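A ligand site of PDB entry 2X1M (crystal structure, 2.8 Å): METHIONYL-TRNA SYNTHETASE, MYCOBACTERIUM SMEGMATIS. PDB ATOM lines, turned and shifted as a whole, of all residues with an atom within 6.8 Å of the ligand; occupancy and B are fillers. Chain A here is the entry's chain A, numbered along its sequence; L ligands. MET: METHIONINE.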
ATOM      1  N   THR A  18      17.131   1.753  11.398  1.00  0.00           N
ATOM      2  CA  THR A  18      18.451   1.202  11.713  1.00  0.00           C
ATOM      3  C   THR A  18      19.314   1.250  10.446  1.00  0.00           C
ATOM      4  O   THR A  18      18.794   1.467   9.346  1.00  0.00           O
ATOM      5  CB  THR A  18      18.403  -0.269  12.200  1.00  0.00           C
ATOM      6  OG1 THR A  18      18.170  -1.157  11.093  1.00  0.00           O
ATOM      7  CG2 THR A  18      17.309  -0.468  13.239  1.00  0.00           C
ATOM      8  N   ALA A  19      20.610   1.037  10.603  1.00  0.00           N
ATOM      9  CA  ALA A  19      21.506   0.902   9.462  1.00  0.00           C
ATOM     10  C   ALA A  19      21.254  -0.438   8.780  1.00  0.00           C
ATOM     11  O   ALA A  19      21.162  -1.474   9.449  1.00  0.00           O
ATOM     12  CB  ALA A  19      22.956   1.020   9.899  1.00  0.00           C
ATOM     13  N   ILE A  20      21.125  -0.412   7.457  1.00  0.00           N
ATOM     14  CA  ILE A  20      20.919  -1.633   6.676  1.00  0.00           C
ATOM     15  C   ILE A  20      22.273  -2.268   6.314  1.00  0.00           C
ATOM     16  O   ILE A  20      22.971  -1.810   5.420  1.00  0.00           O
ATOM     17  CB  ILE A  20      20.027  -1.382   5.416  1.00  0.00           C
ATOM     18  CG1 ILE A  20      20.607  -0.278   4.534  1.00  0.00           C
ATOM     19  CG2 ILE A  20      18.603  -1.039   5.833  1.00  0.00           C
ATOM     20  CD1 ILE A  20      20.111  -0.319   3.091  1.00  0.00           C
ATOM     21  N   ALA A  21      22.624  -3.330   7.047  1.00  0.00           N
ATOM     22  CA  ALA A  21      23.965  -3.913   6.971  1.00  0.00           C
ATOM     23  C   ALA A  21      24.202  -4.771   5.729  1.00  0.00           C
ATOM     24  O   ALA A  21      23.258  -5.237   5.092  1.00  0.00           O
ATOM     25  CB  ALA A  21      24.264  -4.713   8.237  1.00  0.00           C
ATOM     26  N   TYR A  22      25.477  -4.963   5.387  1.00  0.00           N
ATOM     27  CA  TYR A  22      25.881  -5.856   4.301  1.00  0.00           C
ATOM     28  C   TYR A  22      25.679  -7.311   4.725  1.00  0.00           C
ATOM     29  O   TYR A  22      26.239  -7.745   5.734  1.00  0.00           O
ATOM     30  CB  TYR A  22      27.341  -5.640   3.905  1.00  0.00           C
ATOM     31  CG  TYR A  22      27.693  -4.229   3.476  1.00  0.00           C
ATOM     32  CD1 TYR A  22      28.501  -3.417   4.270  1.00  0.00           C
ATOM     33  CD2 TYR A  22      27.218  -3.708   2.261  1.00  0.00           C
ATOM     34  CE1 TYR A  22      28.826  -2.115   3.874  1.00  0.00           C
ATOM     35  CE2 TYR A  22      27.536  -2.409   1.860  1.00  0.00           C
ATOM     36  CZ  TYR A  22      28.338  -1.620   2.673  1.00  0.00           C
ATOM     37  OH  TYR A  22      28.663  -0.347   2.291  1.00  0.00           O
ATOM     38  N   PRO A  23      24.890  -8.072   3.952  1.00  0.00           N
ATOM     39  CA  PRO A  23      24.722  -9.496   4.230  1.00  0.00           C
ATOM     40  C   PRO A  23      25.820 -10.339   3.562  1.00  0.00           C
ATOM     41  O   PRO A  23      25.532 -11.202   2.742  1.00  0.00           O
ATOM     42  CB  PRO A  23      23.340  -9.810   3.638  1.00  0.00           C
ATOM     43  CG  PRO A  23      23.153  -8.818   2.549  1.00  0.00           C
ATOM     44  CD  PRO A  23      24.037  -7.630   2.826  1.00  0.00           C
ATOM     45  N   HIS A  31      25.342  -5.704  15.310  1.00  0.00           N
ATOM     46  CA  HIS A  31      24.056  -5.625  14.617  1.00  0.00           C
ATOM     47  C   HIS A  31      22.901  -5.846  15.593  1.00  0.00           C
ATOM     48  O   HIS A  31      21.966  -5.053  15.637  1.00  0.00           O
ATOM     49  CB  HIS A  31      23.988  -6.650  13.476  1.00  0.00           C
ATOM     50  CG  HIS A  31      25.022  -6.426  12.417  1.00  0.00           C
ATOM     51  ND1 HIS A  31      25.951  -7.388  12.081  1.00  0.00           N
ATOM     52  CD2 HIS A  31      25.275  -5.372  11.612  1.00  0.00           C
ATOM     53  CE1 HIS A  31      26.731  -6.932  11.113  1.00  0.00           C
ATOM     54  NE2 HIS A  31      26.345  -5.706  10.816  1.00  0.00           N
ATOM     55  N   THR A  58      18.773  -4.774   4.924  1.00  0.00           N
ATOM     56  CA  THR A  58      20.101  -5.108   4.406  1.00  0.00           C
ATOM     57  C   THR A  58      20.494  -4.267   3.188  1.00  0.00           C
ATOM     58  O   THR A  58      19.628  -3.760   2.463  1.00  0.00           O
ATOM     59  CB  THR A  58      20.194  -6.607   4.012  1.00  0.00           C
ATOM     60  OG1 THR A  58      19.130  -6.948   3.116  1.00  0.00           O
ATOM     61  CG2 THR A  58      20.116  -7.500   5.252  1.00  0.00           C
ATOM     62  N   ASP A  59      21.793  -4.117   2.983  1.00  0.00           N
ATOM     63  CA  ASP A  59      22.343  -3.432   1.818  1.00  0.00           C
ATOM     64  C   ASP A  59      23.076  -4.471   0.967  1.00  0.00           C
ATOM     65  O   ASP A  59      24.252  -4.781   1.208  1.00  0.00           O
ATOM     66  CB  ASP A  59      23.292  -2.318   2.268  1.00  0.00           C
ATOM     67  CG  ASP A  59      23.812  -1.479   1.122  1.00  0.00           C
ATOM     68  OD1 ASP A  59      23.217  -1.491   0.022  1.00  0.00           O
ATOM     69  OD2 ASP A  59      24.837  -0.794   1.327  1.00  0.00           O
ATOM     70  N   VAL A  60      22.379  -4.996  -0.037  1.00  0.00           N
ATOM     71  CA  VAL A  60      22.816  -6.190  -0.770  1.00  0.00           C
ATOM     72  C   VAL A  60      23.800  -5.951  -1.924  1.00  0.00           C
ATOM     73  O   VAL A  60      24.427  -6.887  -2.407  1.00  0.00           O
ATOM     74  CB  VAL A  60      21.606  -7.031  -1.277  1.00  0.00           C
ATOM     75  CG1 VAL A  60      20.727  -7.475  -0.115  1.00  0.00           C
ATOM     76  CG2 VAL A  60      20.791  -6.262  -2.310  1.00  0.00           C
ATOM     77  N   LYS A  64      31.925  -5.356  -2.173  1.00  0.00           N
ATOM     78  CA  LYS A  64      32.085  -6.203  -0.994  1.00  0.00           C
ATOM     79  C   LYS A  64      31.215  -7.457  -1.105  1.00  0.00           C
ATOM     80  O   LYS A  64      31.666  -8.560  -0.813  1.00  0.00           O
ATOM     81  CB  LYS A  64      31.743  -5.420   0.268  1.00  0.00           C
ATOM     82  CG  LYS A  64      32.175  -6.081   1.570  1.00  0.00           C
ATOM     83  CD  LYS A  64      32.129  -5.104   2.728  1.00  0.00           C
ATOM     84  CE  LYS A  64      32.619  -5.733   4.024  1.00  0.00           C
ATOM     85  NZ  LYS A  64      31.523  -6.425   4.761  1.00  0.00           N
ATOM     86  N   ASP A 139      35.280  -1.264   3.481  1.00  0.00           N
ATOM     87  CA  ASP A 139      34.564  -0.107   4.013  1.00  0.00           C
ATOM     88  C   ASP A 139      33.567   0.445   2.994  1.00  0.00           C
ATOM     89  O   ASP A 139      32.639   1.165   3.372  1.00  0.00           O
ATOM     90  CB  ASP A 139      35.554   0.986   4.419  1.00  0.00           C
ATOM     91  CG  ASP A 139      36.515   0.538   5.507  1.00  0.00           C
ATOM     92  OD1 ASP A 139      36.058   0.052   6.560  1.00  0.00           O
ATOM     93  OD2 ASP A 139      37.735   0.694   5.301  1.00  0.00           O
ATOM     94  N   VAL A 238      27.343   2.276  -4.011  1.00  0.00           N
ATOM     95  CA  VAL A 238      26.562   1.510  -3.038  1.00  0.00           C
ATOM     96  C   VAL A 238      25.948   2.350  -1.907  1.00  0.00           C
ATOM     97  O   VAL A 238      24.845   2.053  -1.447  1.00  0.00           O
ATOM     98  CB  VAL A 238      27.387   0.307  -2.471  1.00  0.00           C
ATOM     99  CG1 VAL A 238      28.605   0.792  -1.673  1.00  0.00           C
ATOM    100  CG2 VAL A 238      26.510  -0.615  -1.624  1.00  0.00           C
ATOM    101  N   TRP A 239      26.643   3.400  -1.487  1.00  0.00           N
ATOM    102  CA  TRP A 239      26.153   4.267  -0.413  1.00  0.00           C
ATOM    103  C   TRP A 239      24.995   5.186  -0.838  1.00  0.00           C
ATOM    104  O   TRP A 239      24.074   5.409  -0.050  1.00  0.00           O
ATOM    105  CB  TRP A 239      27.296   5.059   0.222  1.00  0.00           C
ATOM    106  CG  TRP A 239      27.976   4.273   1.287  1.00  0.00           C
ATOM    107  CD1 TRP A 239      29.145   3.568   1.168  1.00  0.00           C
ATOM    108  CD2 TRP A 239      27.529   4.060   2.631  1.00  0.00           C
ATOM    109  NE1 TRP A 239      29.452   2.951   2.355  1.00  0.00           N
ATOM    110  CE2 TRP A 239      28.470   3.237   3.265  1.00  0.00           C
ATOM    111  CE3 TRP A 239      26.409   4.507   3.356  1.00  0.00           C
ATOM    112  CZ2 TRP A 239      28.337   2.845   4.603  1.00  0.00           C
ATOM    113  CZ3 TRP A 239      26.275   4.106   4.682  1.00  0.00           C
ATOM    114  CH2 TRP A 239      27.232   3.287   5.294  1.00  0.00           C
ATOM    115  N   ASP A 241      22.965   4.324  -3.144  1.00  0.00           N
ATOM    116  CA  ASP A 241      21.950   3.268  -3.171  1.00  0.00           C
ATOM    117  C   ASP A 241      21.454   2.948  -1.765  1.00  0.00           C
ATOM    118  O   ASP A 241      20.249   2.896  -1.523  1.00  0.00           O
ATOM    119  CB  ASP A 241      22.518   2.021  -3.846  1.00  0.00           C
ATOM    120  CG  ASP A 241      21.605   0.806  -3.729  1.00  0.00           C
ATOM    121  OD1 ASP A 241      20.368   0.965  -3.853  1.00  0.00           O
ATOM    122  OD2 ASP A 241      22.123  -0.304  -3.505  1.00  0.00           O
ATOM    123  N   ALA A 242      22.392   2.750  -0.830  1.00  0.00           N
ATOM    124  CA  ALA A 242      22.073   2.340   0.539  1.00  0.00           C
ATOM    125  C   ALA A 242      21.269   3.375   1.313  1.00  0.00           C
ATOM    126  O   ALA A 242      20.249   3.044   1.905  1.00  0.00           O
ATOM    127  CB  ALA A 242      23.347   2.003   1.298  1.00  0.00           C
ATOM    128  N   LEU A 243      21.736   4.624   1.289  1.00  0.00           N
ATOM    129  CA  LEU A 243      21.130   5.697   2.077  1.00  0.00           C
ATOM    130  C   LEU A 243      19.687   6.021   1.685  1.00  0.00           C
ATOM    131  O   LEU A 243      18.887   6.424   2.523  1.00  0.00           O
ATOM    132  CB  LEU A 243      21.994   6.960   2.020  1.00  0.00           C
ATOM    133  CG  LEU A 243      23.315   6.979   2.794  1.00  0.00           C
ATOM    134  CD1 LEU A 243      24.233   8.058   2.252  1.00  0.00           C
ATOM    135  CD2 LEU A 243      23.095   7.169   4.288  1.00  0.00           C
ATOM    136  N   THR A 244      19.374   5.823   0.399  1.00  0.00           N
ATOM    137  CA  THR A 244      18.041   6.097  -0.133  1.00  0.00           C
ATOM    138  C   THR A 244      16.953   5.169   0.444  1.00  0.00           C
ATOM    139  O   THR A 244      15.768   5.465   0.360  1.00  0.00           O
ATOM    140  CB  THR A 244      18.024   6.039  -1.686  1.00  0.00           C
ATOM    141  OG1 THR A 244      19.108   6.837  -2.198  1.00  0.00           O
ATOM    142  CG2 THR A 244      16.723   6.572  -2.260  1.00  0.00           C
ATOM    143  N   ASN A 245      17.376   4.055   1.054  1.00  0.00           N
ATOM    144  CA  ASN A 245      16.443   3.109   1.676  1.00  0.00           C
ATOM    145  C   ASN A 245      15.487   3.771   2.670  1.00  0.00           C
ATOM    146  O   ASN A 245      14.311   3.413   2.739  1.00  0.00           O
ATOM    147  CB  ASN A 245      17.177   1.937   2.331  1.00  0.00           C
ATOM    148  CG  ASN A 245      17.609   2.231   3.759  1.00  0.00           C
ATOM    149  OD1 ASN A 245      16.997   1.743   4.709  1.00  0.00           O
ATOM    150  ND2 ASN A 245      18.645   3.050   3.921  1.00  0.00           N
ATOM    151  N   TYR A 246      16.005   4.738   3.432  1.00  0.00           N
ATOM    152  CA  TYR A 246      15.226   5.474   4.414  1.00  0.00           C
ATOM    153  C   TYR A 246      14.067   6.231   3.773  1.00  0.00           C
ATOM    154  O   TYR A 246      13.040   6.471   4.401  1.00  0.00           O
ATOM    155  CB  TYR A 246      16.130   6.448   5.195  1.00  0.00           C
ATOM    156  CG  TYR A 246      17.364   5.824   5.831  1.00  0.00           C
ATOM    157  CD1 TYR A 246      17.271   4.637   6.572  1.00  0.00           C
ATOM    158  CD2 TYR A 246      18.607   6.429   5.715  1.00  0.00           C
ATOM    159  CE1 TYR A 246      18.400   4.082   7.161  1.00  0.00           C
ATOM    160  CE2 TYR A 246      19.735   5.874   6.304  1.00  0.00           C
ATOM    161  CZ  TYR A 246      19.624   4.702   7.026  1.00  0.00           C
ATOM    162  OH  TYR A 246      20.745   4.145   7.609  1.00  0.00           O
ATOM    163  N   ILE A 271      22.591   4.352  14.042  1.00  0.00           N
ATOM    164  CA  ILE A 271      23.753   3.808  13.341  1.00  0.00           C
ATOM    165  C   ILE A 271      24.932   3.558  14.290  1.00  0.00           C
ATOM    166  O   ILE A 271      24.978   4.107  15.388  1.00  0.00           O
ATOM    167  CB  ILE A 271      24.244   4.743  12.207  1.00  0.00           C
ATOM    168  CG1 ILE A 271      24.620   6.127  12.757  1.00  0.00           C
ATOM    169  CG2 ILE A 271      23.196   4.845  11.084  1.00  0.00           C
ATOM    170  CD1 ILE A 271      25.670   6.860  11.958  1.00  0.00           C
ATOM    171  N   ASP A 274      31.080   3.912  13.119  1.00  0.00           N
ATOM    172  CA  ASP A 274      32.017   3.711  12.007  1.00  0.00           C
ATOM    173  C   ASP A 274      31.479   4.189  10.655  1.00  0.00           C
ATOM    174  O   ASP A 274      32.236   4.327   9.692  1.00  0.00           O
ATOM    175  CB  ASP A 274      32.462   2.242  11.926  1.00  0.00           C
ATOM    176  CG  ASP A 274      31.316   1.297  11.588  1.00  0.00           C
ATOM    177  OD1 ASP A 274      30.171   1.534  12.029  1.00  0.00           O
ATOM    178  OD2 ASP A 274      31.566   0.299  10.875  1.00  0.00           O
ATOM    179  N   ILE A 275      30.177   4.450  10.588  1.00  0.00           N
ATOM    180  CA  ILE A 275      29.529   4.909   9.356  1.00  0.00           C
ATOM    181  C   ILE A 275      28.834   6.258   9.548  1.00  0.00           C
ATOM    182  O   ILE A 275      27.823   6.555   8.889  1.00  0.00           O
ATOM    183  CB  ILE A 275      28.559   3.841   8.792  1.00  0.00           C
ATOM    184  CG1 ILE A 275      27.535   3.413   9.846  1.00  0.00           C
ATOM    185  CG2 ILE A 275      29.337   2.644   8.264  1.00  0.00           C
ATOM    186  CD1 ILE A 275      26.278   2.768   9.275  1.00  0.00           C
ATOM    187  N   PHE A 278      28.943   9.117   6.481  1.00  0.00           N
ATOM    188  CA  PHE A 278      27.952   8.885   5.436  1.00  0.00           C
ATOM    189  C   PHE A 278      26.604   9.515   5.792  1.00  0.00           C
ATOM    190  O   PHE A 278      25.952  10.107   4.934  1.00  0.00           O
ATOM    191  CB  PHE A 278      27.771   7.387   5.180  1.00  0.00           C
ATOM    192  CG  PHE A 278      29.033   6.664   4.810  1.00  0.00           C
ATOM    193  CD1 PHE A 278      29.747   5.948   5.762  1.00  0.00           C
ATOM    194  CD2 PHE A 278      29.501   6.692   3.488  1.00  0.00           C
ATOM    195  CE1 PHE A 278      30.909   5.271   5.416  1.00  0.00           C
ATOM    196  CE2 PHE A 278      30.672   6.025   3.142  1.00  0.00           C
ATOM    197  CZ  PHE A 278      31.379   5.308   4.106  1.00  0.00           C
ATOM    198  N   HIS A 279      26.217   9.388   7.051  1.00  0.00           N
ATOM    199  CA  HIS A 279      24.899   9.819   7.530  1.00  0.00           C
ATOM    200  C   HIS A 279      24.822  11.293   7.914  1.00  0.00           C
ATOM    201  O   HIS A 279      23.741  11.880   7.851  1.00  0.00           O
ATOM    202  CB  HIS A 279      24.449   8.943   8.702  1.00  0.00           C
ATOM    203  CG  HIS A 279      24.026   7.569   8.295  1.00  0.00           C
ATOM    204  ND1 HIS A 279      24.917   6.532   8.113  1.00  0.00           N
ATOM    205  CD2 HIS A 279      22.797   7.056   8.042  1.00  0.00           C
ATOM    206  CE1 HIS A 279      24.262   5.446   7.760  1.00  0.00           C
ATOM    207  NE2 HIS A 279      22.972   5.734   7.715  1.00  0.00           N
HETATM  208  N   MET L   1      25.604  -1.379   4.697  1.00  0.00           N
HETATM  209  CA  MET L   1      26.182  -0.385   5.609  1.00  0.00           C
HETATM  210  C   MET L   1      27.054  -1.061   6.679  1.00  0.00           C
HETATM  211  O   MET L   1      27.853  -0.400   7.348  1.00  0.00           O
HETATM  212  CB  MET L   1      25.079   0.441   6.272  1.00  0.00           C
HETATM  213  CG  MET L   1      24.237   1.258   5.305  1.00  0.00           C
HETATM  214  SD  MET L   1      23.177   2.421   6.170  1.00  0.00           S
HETATM  215  CE  MET L   1      22.291   3.148   4.802  1.00  0.00           C
HETATM  216  OXT MET L   1      26.968  -2.264   6.900  1.00  0.00           O
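Ala 19 touches the ligand. CA of Ala 21 touches OXT of the ligand, at 3.4 Å. Trp 239 touches the ligand. Ala 242 touches the ligand (O to CE, 3.5 Å). Leu 243 touches the ligand (N to CE, 3.9 Å). Asn 245 touches the ligand. CG2 of Ile 275 touches O of the ligand, at 3.5 Å. Hydrophobic or aromatic side chains that line the ligand: Ala 19, Ile 20, Ala 21, Tyr 22, Trp 239, Ala 242, Tyr 246, Ile 275 and His 279. The nearest printed residue that does not touch the ligand is Asp 274 (5.2 Å).
The backbone NH (N) of Ile 20 sits close to a sulfur (SD) of the ligand (3.7 Å). O of Ile 20 is in hydrogen-bond range of N of the ligand, at 2.8 Å. An oxygen (OXT) of the ligand sits close to the backbone NH (N) of Tyr 22 (3.4 Å). The side-chain hydroxyl (OH) of Tyr 246 sits close to a sulfur (SD) of the ligand (3.3 Å). The side-chain carboxylate of Asp 59 lies within salt-bridge range of a nitrogen (N) of the ligand (3.5 Å). A ring nitrogen (NE2) of His 279 sits close to a sulfur (SD) of the ligand (3.7 Å).
OH of Tyr 22 lies within hydrogen-bond range of NE1 of Trp 239 (3.4 Å). The side-chain hydroxyl of Tyr 246 sits at hydrogen-bond distance from a ring nitrogen (NE2) of His 279, 2.7 Å away. The backbone carbonyl oxygen of Ala 21 sits at hydrogen-bond distance from the backbone NH of Asp 59. ND1 of His 279 is in hydrogen-bond range of O of Ile 275, at 3.0 Å. The side-chain amide nitrogen (ND2) of Asn 245 lies within hydrogen-bond range of the backbone carbonyl oxygen (O) of Ala 242 (2.6 Å).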
